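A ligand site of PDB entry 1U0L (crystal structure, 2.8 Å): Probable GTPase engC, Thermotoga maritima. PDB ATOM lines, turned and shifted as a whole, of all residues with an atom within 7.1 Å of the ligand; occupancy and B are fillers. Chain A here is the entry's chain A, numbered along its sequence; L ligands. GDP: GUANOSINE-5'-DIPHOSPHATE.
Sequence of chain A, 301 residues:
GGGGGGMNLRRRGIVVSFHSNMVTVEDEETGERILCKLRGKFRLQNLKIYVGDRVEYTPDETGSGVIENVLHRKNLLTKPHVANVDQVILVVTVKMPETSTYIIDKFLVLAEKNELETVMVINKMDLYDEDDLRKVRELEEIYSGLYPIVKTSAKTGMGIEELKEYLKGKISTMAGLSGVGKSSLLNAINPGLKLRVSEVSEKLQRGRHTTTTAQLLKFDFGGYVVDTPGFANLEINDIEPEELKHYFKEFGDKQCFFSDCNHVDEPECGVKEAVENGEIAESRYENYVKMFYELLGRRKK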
ATOM      1  N   VAL A  91     -26.537  -3.754  16.360  1.00  0.00           N
ATOM      2  CA  VAL A  91     -26.301  -2.741  15.357  1.00  0.00           C
ATOM      3  C   VAL A  91     -27.552  -2.563  14.518  1.00  0.00           C
ATOM      4  O   VAL A  91     -28.091  -3.510  13.950  1.00  0.00           O
ATOM      5  CB  VAL A  91     -25.075  -3.081  14.491  1.00  0.00           C
ATOM      6  CG1 VAL A  91     -24.964  -2.127  13.337  1.00  0.00           C
ATOM      7  CG2 VAL A  91     -23.838  -2.956  15.340  1.00  0.00           C
ATOM      8  N   MET A  96     -30.177   2.565   4.349  1.00  0.00           N
ATOM      9  CA  MET A  96     -29.603   1.360   3.764  1.00  0.00           C
ATOM     10  C   MET A  96     -30.219   0.052   4.288  1.00  0.00           C
ATOM     11  O   MET A  96     -31.354  -0.252   3.928  1.00  0.00           O
ATOM     12  CB  MET A  96     -28.088   1.358   3.911  1.00  0.00           C
ATOM     13  CG  MET A  96     -27.399   2.219   2.871  1.00  0.00           C
ATOM     14  SD  MET A  96     -28.060   1.940   1.209  1.00  0.00           S
ATOM     15  CE  MET A  96     -29.008   3.477   0.984  1.00  0.00           C
ATOM     16  N   PRO A  97     -29.517  -0.719   5.137  1.00  0.00           N
ATOM     17  CA  PRO A  97     -30.374  -1.939   5.447  1.00  0.00           C
ATOM     18  C   PRO A  97     -31.815  -1.784   5.955  1.00  0.00           C
ATOM     19  O   PRO A  97     -32.589  -2.735   5.884  1.00  0.00           O
ATOM     20  CB  PRO A  97     -29.499  -2.681   6.429  1.00  0.00           C
ATOM     21  CG  PRO A  97     -28.119  -2.403   5.865  1.00  0.00           C
ATOM     22  CD  PRO A  97     -28.165  -0.917   5.491  1.00  0.00           C
ATOM     23  N   ASN A 123     -25.885   2.615  13.432  1.00  0.00           N
ATOM     24  CA  ASN A 123     -24.704   2.800  12.581  1.00  0.00           C
ATOM     25  C   ASN A 123     -24.922   3.543  11.244  1.00  0.00           C
ATOM     26  O   ASN A 123     -26.053   3.881  10.874  1.00  0.00           O
ATOM     27  CB  ASN A 123     -24.096   1.423  12.305  1.00  0.00           C
ATOM     28  CG  ASN A 123     -22.735   1.499  11.640  1.00  0.00           C
ATOM     29  OD1 ASN A 123     -22.397   0.669  10.785  1.00  0.00           O
ATOM     30  ND2 ASN A 123     -21.932   2.498  12.039  1.00  0.00           N
ATOM     31  N   LYS A 124     -23.834   3.797  10.520  1.00  0.00           N
ATOM     32  CA  LYS A 124     -23.895   4.465   9.221  1.00  0.00           C
ATOM     33  C   LYS A 124     -24.416   5.894   9.302  1.00  0.00           C
ATOM     34  O   LYS A 124     -25.080   6.377   8.378  1.00  0.00           O
ATOM     35  CB  LYS A 124     -24.809   3.688   8.263  1.00  0.00           C
ATOM     36  CG  LYS A 124     -24.388   2.257   7.937  1.00  0.00           C
ATOM     37  CD  LYS A 124     -24.831   1.888   6.525  1.00  0.00           C
ATOM     38  CE  LYS A 124     -25.132   0.395   6.330  1.00  0.00           C
ATOM     39  NZ  LYS A 124     -23.903  -0.409   6.265  1.00  0.00           N
ATOM     40  N   MET A 125     -24.118   6.587  10.400  1.00  0.00           N
ATOM     41  CA  MET A 125     -24.589   7.949  10.576  1.00  0.00           C
ATOM     42  C   MET A 125     -24.084   8.864   9.474  1.00  0.00           C
ATOM     43  O   MET A 125     -24.758   9.820   9.088  1.00  0.00           O
ATOM     44  CB  MET A 125     -24.148   8.492  11.927  1.00  0.00           C
ATOM     45  CG  MET A 125     -24.755   7.780  13.140  1.00  0.00           C
ATOM     46  SD  MET A 125     -26.487   8.165  13.470  1.00  0.00           S
ATOM     47  CE  MET A 125     -26.368   9.902  13.745  1.00  0.00           C
ATOM     48  N   ASP A 126     -22.895   8.564   8.961  1.00  0.00           N
ATOM     49  CA  ASP A 126     -22.298   9.398   7.922  1.00  0.00           C
ATOM     50  C   ASP A 126     -23.132   9.466   6.661  1.00  0.00           C
ATOM     51  O   ASP A 126     -22.939  10.343   5.827  1.00  0.00           O
ATOM     52  CB  ASP A 126     -20.906   8.866   7.558  1.00  0.00           C
ATOM     53  CG  ASP A 126     -20.946   7.452   7.043  1.00  0.00           C
ATOM     54  OD1 ASP A 126     -21.094   6.531   7.872  1.00  0.00           O
ATOM     55  OD2 ASP A 126     -20.852   7.256   5.811  1.00  0.00           O
ATOM     56  N   LEU A 127     -24.071   8.536   6.531  1.00  0.00           N
ATOM     57  CA  LEU A 127     -24.910   8.458   5.341  1.00  0.00           C
ATOM     58  C   LEU A 127     -26.248   9.192   5.462  1.00  0.00           C
ATOM     59  O   LEU A 127     -26.888   9.477   4.463  1.00  0.00           O
ATOM     60  CB  LEU A 127     -25.206   6.984   5.044  1.00  0.00           C
ATOM     61  CG  LEU A 127     -24.805   6.325   3.732  1.00  0.00           C
ATOM     62  CD1 LEU A 127     -23.302   6.433   3.506  1.00  0.00           C
ATOM     63  CD2 LEU A 127     -25.239   4.862   3.798  1.00  0.00           C
ATOM     64  N   THR A 152     -22.923   5.577  15.622  1.00  0.00           N
ATOM     65  CA  THR A 152     -21.616   5.327  15.037  1.00  0.00           C
ATOM     66  C   THR A 152     -21.500   5.436  13.514  1.00  0.00           C
ATOM     67  O   THR A 152     -22.472   5.608  12.793  1.00  0.00           O
ATOM     68  CB  THR A 152     -21.107   3.930  15.412  1.00  0.00           C
ATOM     69  OG1 THR A 152     -21.849   2.940  14.669  1.00  0.00           O
ATOM     70  CG2 THR A 152     -21.315   3.672  16.897  1.00  0.00           C
ATOM     71  N   SER A 153     -20.246   5.338  13.055  1.00  0.00           N
ATOM     72  CA  SER A 153     -19.911   5.320  11.641  1.00  0.00           C
ATOM     73  C   SER A 153     -18.626   4.541  11.526  1.00  0.00           C
ATOM     74  O   SER A 153     -17.563   5.032  11.878  1.00  0.00           O
ATOM     75  CB  SER A 153     -19.686   6.714  11.079  1.00  0.00           C
ATOM     76  OG  SER A 153     -19.381   6.619   9.687  1.00  0.00           O
ATOM     77  N   ALA A 154     -18.721   3.303  11.050  1.00  0.00           N
ATOM     78  CA  ALA A 154     -17.546   2.467  10.881  1.00  0.00           C
ATOM     79  C   ALA A 154     -16.524   3.229  10.031  1.00  0.00           C
ATOM     80  O   ALA A 154     -15.325   3.152  10.280  1.00  0.00           O
ATOM     81  CB  ALA A 154     -17.920   1.164  10.198  1.00  0.00           C
ATOM     82  N   LYS A 155     -17.030   3.962   9.044  1.00  0.00           N
ATOM     83  CA  LYS A 155     -16.187   4.743   8.130  1.00  0.00           C
ATOM     84  C   LYS A 155     -15.530   5.964   8.783  1.00  0.00           C
ATOM     85  O   LYS A 155     -14.308   6.085   8.847  1.00  0.00           O
ATOM     86  CB  LYS A 155     -17.022   5.207   6.936  1.00  0.00           C
ATOM     87  CG  LYS A 155     -17.472   4.100   5.999  1.00  0.00           C
ATOM     88  CD  LYS A 155     -16.298   3.503   5.222  1.00  0.00           C
ATOM     89  CE  LYS A 155     -16.756   2.427   4.244  1.00  0.00           C
ATOM     90  NZ  LYS A 155     -17.710   2.969   3.235  1.00  0.00           N
ATOM     91  N   THR A 156     -16.366   6.901   9.240  1.00  0.00           N
ATOM     92  CA  THR A 156     -15.897   8.119   9.875  1.00  0.00           C
ATOM     93  C   THR A 156     -15.195   7.899  11.210  1.00  0.00           C
ATOM     94  O   THR A 156     -14.343   8.683  11.615  1.00  0.00           O
ATOM     95  CB  THR A 156     -17.065   9.062  10.140  1.00  0.00           C
ATOM     96  OG1 THR A 156     -17.617   9.480   8.895  1.00  0.00           O
ATOM     97  CG2 THR A 156     -16.605  10.271  10.886  1.00  0.00           C
ATOM     98  N   GLY A 157     -15.589   6.825  11.894  1.00  0.00           N
ATOM     99  CA  GLY A 157     -14.988   6.537  13.181  1.00  0.00           C
ATOM    100  C   GLY A 157     -15.853   7.090  14.302  1.00  0.00           C
ATOM    101  O   GLY A 157     -15.589   6.872  15.478  1.00  0.00           O
ATOM    102  N   GLY A 176     -27.634  -8.072  14.399  1.00  0.00           N
ATOM    103  CA  GLY A 176     -28.281  -7.119  13.517  1.00  0.00           C
ATOM    104  C   GLY A 176     -28.435  -7.671  12.108  1.00  0.00           C
ATOM    105  O   GLY A 176     -27.755  -8.624  11.733  1.00  0.00           O
ATOM    106  N   LEU A 177     -29.349  -7.086  11.344  1.00  0.00           N
ATOM    107  CA  LEU A 177     -29.609  -7.494   9.965  1.00  0.00           C
ATOM    108  C   LEU A 177     -28.364  -7.435   9.066  1.00  0.00           C
ATOM    109  O   LEU A 177     -27.518  -6.534   9.198  1.00  0.00           O
ATOM    110  CB  LEU A 177     -30.713  -6.630   9.365  1.00  0.00           C
ATOM    111  CG  LEU A 177     -32.140  -6.724   9.937  1.00  0.00           C
ATOM    112  CD1 LEU A 177     -32.972  -5.626   9.302  1.00  0.00           C
ATOM    113  CD2 LEU A 177     -32.770  -8.083   9.676  1.00  0.00           C
ATOM    114  N   SER A 178     -28.248  -8.389   8.149  1.00  0.00           N
ATOM    115  CA  SER A 178     -27.106  -8.448   7.238  1.00  0.00           C
ATOM    116  C   SER A 178     -26.945  -7.142   6.508  1.00  0.00           C
ATOM    117  O   SER A 178     -27.897  -6.630   5.943  1.00  0.00           O
ATOM    118  CB  SER A 178     -27.306  -9.550   6.208  1.00  0.00           C
ATOM    119  OG  SER A 178     -27.814 -10.708   6.869  1.00  0.00           O
ATOM    120  N   GLY A 179     -25.725  -6.620   6.537  1.00  0.00           N
ATOM    121  CA  GLY A 179     -25.419  -5.374   5.857  1.00  0.00           C
ATOM    122  C   GLY A 179     -25.426  -4.146   6.737  1.00  0.00           C
ATOM    123  O   GLY A 179     -24.887  -3.108   6.366  1.00  0.00           O
ATOM    124  N   VAL A 180     -26.019  -4.277   7.914  1.00  0.00           N
ATOM    125  CA  VAL A 180     -26.136  -3.166   8.849  1.00  0.00           C
ATOM    126  C   VAL A 180     -24.762  -2.592   9.241  1.00  0.00           C
ATOM    127  O   VAL A 180     -24.671  -1.455   9.708  1.00  0.00           O
ATOM    128  CB  VAL A 180     -26.937  -3.609  10.094  1.00  0.00           C
ATOM    129  CG1 VAL A 180     -26.030  -4.367  11.052  1.00  0.00           C
ATOM    130  CG2 VAL A 180     -27.571  -2.425  10.746  1.00  0.00           C
ATOM    131  N   GLY A 181     -23.692  -3.369   9.041  1.00  0.00           N
ATOM    132  CA  GLY A 181     -22.353  -2.897   9.353  1.00  0.00           C
ATOM    133  C   GLY A 181     -21.605  -3.567  10.499  1.00  0.00           C
ATOM    134  O   GLY A 181     -20.610  -3.026  10.980  1.00  0.00           O
ATOM    135  N   LYS A 182     -22.078  -4.731  10.917  1.00  0.00           N
ATOM    136  CA  LYS A 182     -21.470  -5.465  12.039  1.00  0.00           C
ATOM    137  C   LYS A 182     -19.972  -5.752  11.894  1.00  0.00           C
ATOM    138  O   LYS A 182     -19.181  -5.476  12.808  1.00  0.00           O
ATOM    139  CB  LYS A 182     -22.248  -6.767  12.277  1.00  0.00           C
ATOM    140  CG  LYS A 182     -23.732  -6.548  12.592  1.00  0.00           C
ATOM    141  CD  LYS A 182     -24.480  -7.815  13.012  1.00  0.00           C
ATOM    142  CE  LYS A 182     -24.527  -8.868  11.916  1.00  0.00           C
ATOM    143  NZ  LYS A 182     -25.257  -8.505  10.649  1.00  0.00           N
ATOM    144  N   SER A 183     -19.567  -6.280  10.752  1.00  0.00           N
ATOM    145  CA  SER A 183     -18.174  -6.591  10.516  1.00  0.00           C
ATOM    146  C   SER A 183     -17.317  -5.326  10.338  1.00  0.00           C
ATOM    147  O   SER A 183     -16.155  -5.296  10.730  1.00  0.00           O
ATOM    148  CB  SER A 183     -18.042  -7.480   9.283  1.00  0.00           C
ATOM    149  OG  SER A 183     -16.760  -8.098   9.215  1.00  0.00           O
ATOM    150  N   SER A 184     -17.901  -4.271   9.771  1.00  0.00           N
ATOM    151  CA  SER A 184     -17.170  -3.026   9.544  1.00  0.00           C
ATOM    152  C   SER A 184     -16.878  -2.326  10.863  1.00  0.00           C
ATOM    153  O   SER A 184     -15.815  -1.728  11.029  1.00  0.00           O
ATOM    154  CB  SER A 184     -17.958  -2.057   8.655  1.00  0.00           C
ATOM    155  OG  SER A 184     -18.275  -2.631   7.403  1.00  0.00           O
ATOM    156  N   LEU A 185     -17.832  -2.364  11.798  1.00  0.00           N
ATOM    157  CA  LEU A 185     -17.653  -1.724  13.101  1.00  0.00           C
ATOM    158  C   LEU A 185     -16.515  -2.427  13.848  1.00  0.00           C
ATOM    159  O   LEU A 185     -15.649  -1.787  14.437  1.00  0.00           O
ATOM    160  CB  LEU A 185     -18.935  -1.796  13.929  1.00  0.00           C
ATOM    161  CG  LEU A 185     -20.033  -0.798  13.541  1.00  0.00           C
ATOM    162  CD1 LEU A 185     -21.364  -1.178  14.171  1.00  0.00           C
ATOM    163  CD2 LEU A 185     -19.590   0.586  13.997  1.00  0.00           C
ATOM    164  N   LEU A 186     -16.554  -3.759  13.795  1.00  0.00           N
ATOM    165  CA  LEU A 186     -15.564  -4.593  14.432  1.00  0.00           C
ATOM    166  C   LEU A 186     -14.163  -4.168  14.026  1.00  0.00           C
ATOM    167  O   LEU A 186     -13.272  -4.029  14.875  1.00  0.00           O
ATOM    168  CB  LEU A 186     -15.778  -6.051  14.026  1.00  0.00           C
ATOM    169  CG  LEU A 186     -14.905  -7.091  14.718  1.00  0.00           C
ATOM    170  CD1 LEU A 186     -15.046  -6.951  16.216  1.00  0.00           C
ATOM    171  CD2 LEU A 186     -15.331  -8.473  14.280  1.00  0.00           C
ATOM    172  N   LEU A 195     -15.835 -10.347  11.277  1.00  0.00           N
ATOM    173  CA  LEU A 195     -16.819 -11.409  11.425  1.00  0.00           C
ATOM    174  C   LEU A 195     -16.551 -12.531  10.437  1.00  0.00           C
ATOM    175  O   LEU A 195     -15.774 -12.359   9.499  1.00  0.00           O
ATOM    176  CB  LEU A 195     -18.214 -10.856  11.177  1.00  0.00           C
ATOM    177  CG  LEU A 195     -18.711  -9.874  12.236  1.00  0.00           C
ATOM    178  CD1 LEU A 195     -19.978  -9.192  11.732  1.00  0.00           C
ATOM    179  CD2 LEU A 195     -18.972 -10.607  13.549  1.00  0.00           C
ATOM    180  N   PRO A 229     -22.119 -13.688  14.192  1.00  0.00           N
ATOM    181  CA  PRO A 229     -23.128 -12.848  14.859  1.00  0.00           C
ATOM    182  C   PRO A 229     -24.143 -13.608  15.685  1.00  0.00           C
ATOM    183  O   PRO A 229     -24.391 -14.801  15.454  1.00  0.00           O
ATOM    184  CB  PRO A 229     -23.804 -12.094  13.703  1.00  0.00           C
ATOM    185  CG  PRO A 229     -22.817 -12.180  12.597  1.00  0.00           C
ATOM    186  CD  PRO A 229     -22.282 -13.580  12.732  1.00  0.00           C
HETATM  187  PB  GDP L   1     -22.523  -6.817   8.259  1.00  0.00           P
HETATM  188  O1B GDP L   1     -23.448  -6.215   9.280  1.00  0.00           O
HETATM  189  O2B GDP L   1     -23.167  -7.906   7.416  1.00  0.00           O
HETATM  190  O3B GDP L   1     -21.194  -7.323   8.860  1.00  0.00           O
HETATM  191  O3A GDP L   1     -22.141  -5.586   7.202  1.00  0.00           O
HETATM  192  PA  GDP L   1     -20.732  -5.089   6.701  1.00  0.00           P
HETATM  193  O1A GDP L   1     -20.102  -6.085   5.784  1.00  0.00           O
HETATM  194  O2A GDP L   1     -19.863  -4.682   7.889  1.00  0.00           O
HETATM  195  O5' GDP L   1     -21.074  -3.728   5.903  1.00  0.00           O
HETATM  196  C5' GDP L   1     -21.886  -3.802   4.721  1.00  0.00           C
HETATM  197  C4' GDP L   1     -21.511  -2.714   3.765  1.00  0.00           C
HETATM  198  O4' GDP L   1     -21.827  -1.455   4.410  1.00  0.00           O
HETATM  199  C3' GDP L   1     -20.020  -2.686   3.292  1.00  0.00           C
HETATM  200  O3' GDP L   1     -20.043  -2.551   1.797  1.00  0.00           O
HETATM  201  C2' GDP L   1     -19.437  -1.432   3.950  1.00  0.00           C
HETATM  202  O2' GDP L   1     -18.539  -0.799   3.034  1.00  0.00           O
HETATM  203  C1' GDP L   1     -20.708  -0.606   4.377  1.00  0.00           C
HETATM  204  N9  GDP L   1     -20.673   0.094   5.805  1.00  0.00           N
HETATM  205  C8  GDP L   1     -20.546  -0.526   7.008  1.00  0.00           C
HETATM  206  N7  GDP L   1     -20.569   0.379   8.017  1.00  0.00           N
HETATM  207  C5  GDP L   1     -20.719   1.616   7.394  1.00  0.00           C
HETATM  208  C6  GDP L   1     -20.817   2.925   7.956  1.00  0.00           C
HETATM  209  O6  GDP L   1     -20.790   3.204   9.158  1.00  0.00           O
HETATM  210  N1  GDP L   1     -20.966   3.943   6.993  1.00  0.00           N
HETATM  211  C2  GDP L   1     -21.012   3.689   5.635  1.00  0.00           C
HETATM  212  N2  GDP L   1     -21.145   4.736   4.807  1.00  0.00           N
HETATM  213  N3  GDP L   1     -20.920   2.441   5.112  1.00  0.00           N
HETATM  214  C4  GDP L   1     -20.774   1.460   6.040  1.00  0.00           C
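Residues that only touch the ligand: Leu 127 (3.0 Å), Ser 153 (3.4 Å), Lys 155 (3.6 Å), Leu 195 (3.6 Å) and Ser 178 (3.96 Å).
Hydrophobic or aromatic side chains that line the ligand: Leu 127, Ala 154, Val 180 and Leu 195.
15 residues have an atom within 4 Å of the ligand: Asn 123, Lys 124, Asp 126, Leu 127, Ser 153, Ala 154, Lys 155, Ser 178, Gly 179, Val 180, Gly 181, Lys 182, Ser 183, Ser 184 and Leu 195.
NZ of Lys 182 lies within hydrogen-bond range of O of Leu 177.
NZ of Lys 182 is in hydrogen-bond range of O of Gly 176 (2.7 Å).
The backbone NH (N) of Leu 195 sits at hydrogen-bond distance from the side-chain hydroxyl (OG) of Ser 183, at 3.2 Å.
The side-chain carboxylate (OD1) of Asp 126 sits at hydrogen-bond distance from the side-chain hydroxyl (OG) of Ser 153, 2.5 Å away.
The side-chain amide nitrogen (ND2) of Asn 123 sits close to the backbone NH (N) of Ala 154 (3.5 Å).
The side-chain amino group (NZ) of Lys 124 lies within hydrogen-bond range of the backbone carbonyl oxygen (O) of Gly 179, at 2.9 Å.
The side-chain amide nitrogen (ND2) of Asn 123 lies close to the backbone NH (N) of Ser 153.
The side-chain hydroxyl (OG1) of Thr 152 sits at hydrogen-bond distance from the side-chain amide nitrogen (ND2) of Asn 123, at 2.7 Å.
An oxygen (O1B) of the ligand sits at hydrogen-bond distance from the backbone NH (N) of Lys 182.
The side-chain amino group (NZ) of Lys 182 lies within salt-bridge range of an oxygen (O1B) of the ligand, at 3.2 Å.
An oxygen (O2A) of the ligand is in hydrogen-bond range of the backbone NH of Ser 184, 2.7 Å away.
OG of Ser 184 lies within hydrogen-bond range of O2A of the ligand.
O3B of the ligand is in hydrogen-bond range of N of Ser 183, at 2.7 Å.
The side-chain carboxylate (OD2) of Asp 126 sits at hydrogen-bond distance from a nitrogen (N2) of the ligand, at 2.7 Å.
The backbone NH (N) of Ala 154 sits at hydrogen-bond distance from an oxygen (O6) of the ligand (2.8 Å).
An oxygen (O1B) of the ligand lies within hydrogen-bond range of the backbone NH (N) of Gly 181, at 2.9 Å.
An oxygen (O6) of the ligand lies close to the backbone NH (N) of Lys 124 (3.4 Å).
The side-chain amino group of Lys 124 lies within hydrogen-bond range of an oxygen (O4') of the ligand, 3.0 Å away.
N of Gly 179 sits at hydrogen-bond distance from O2B of the ligand (3.0 Å).
The side-chain amide nitrogen of Asn 123 sits at hydrogen-bond distance from an oxygen (O6) of the ligand, 3.2 Å away.
The backbone NH (N) of Val 180 is in hydrogen-bond range of an oxygen (O1B) of the ligand.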
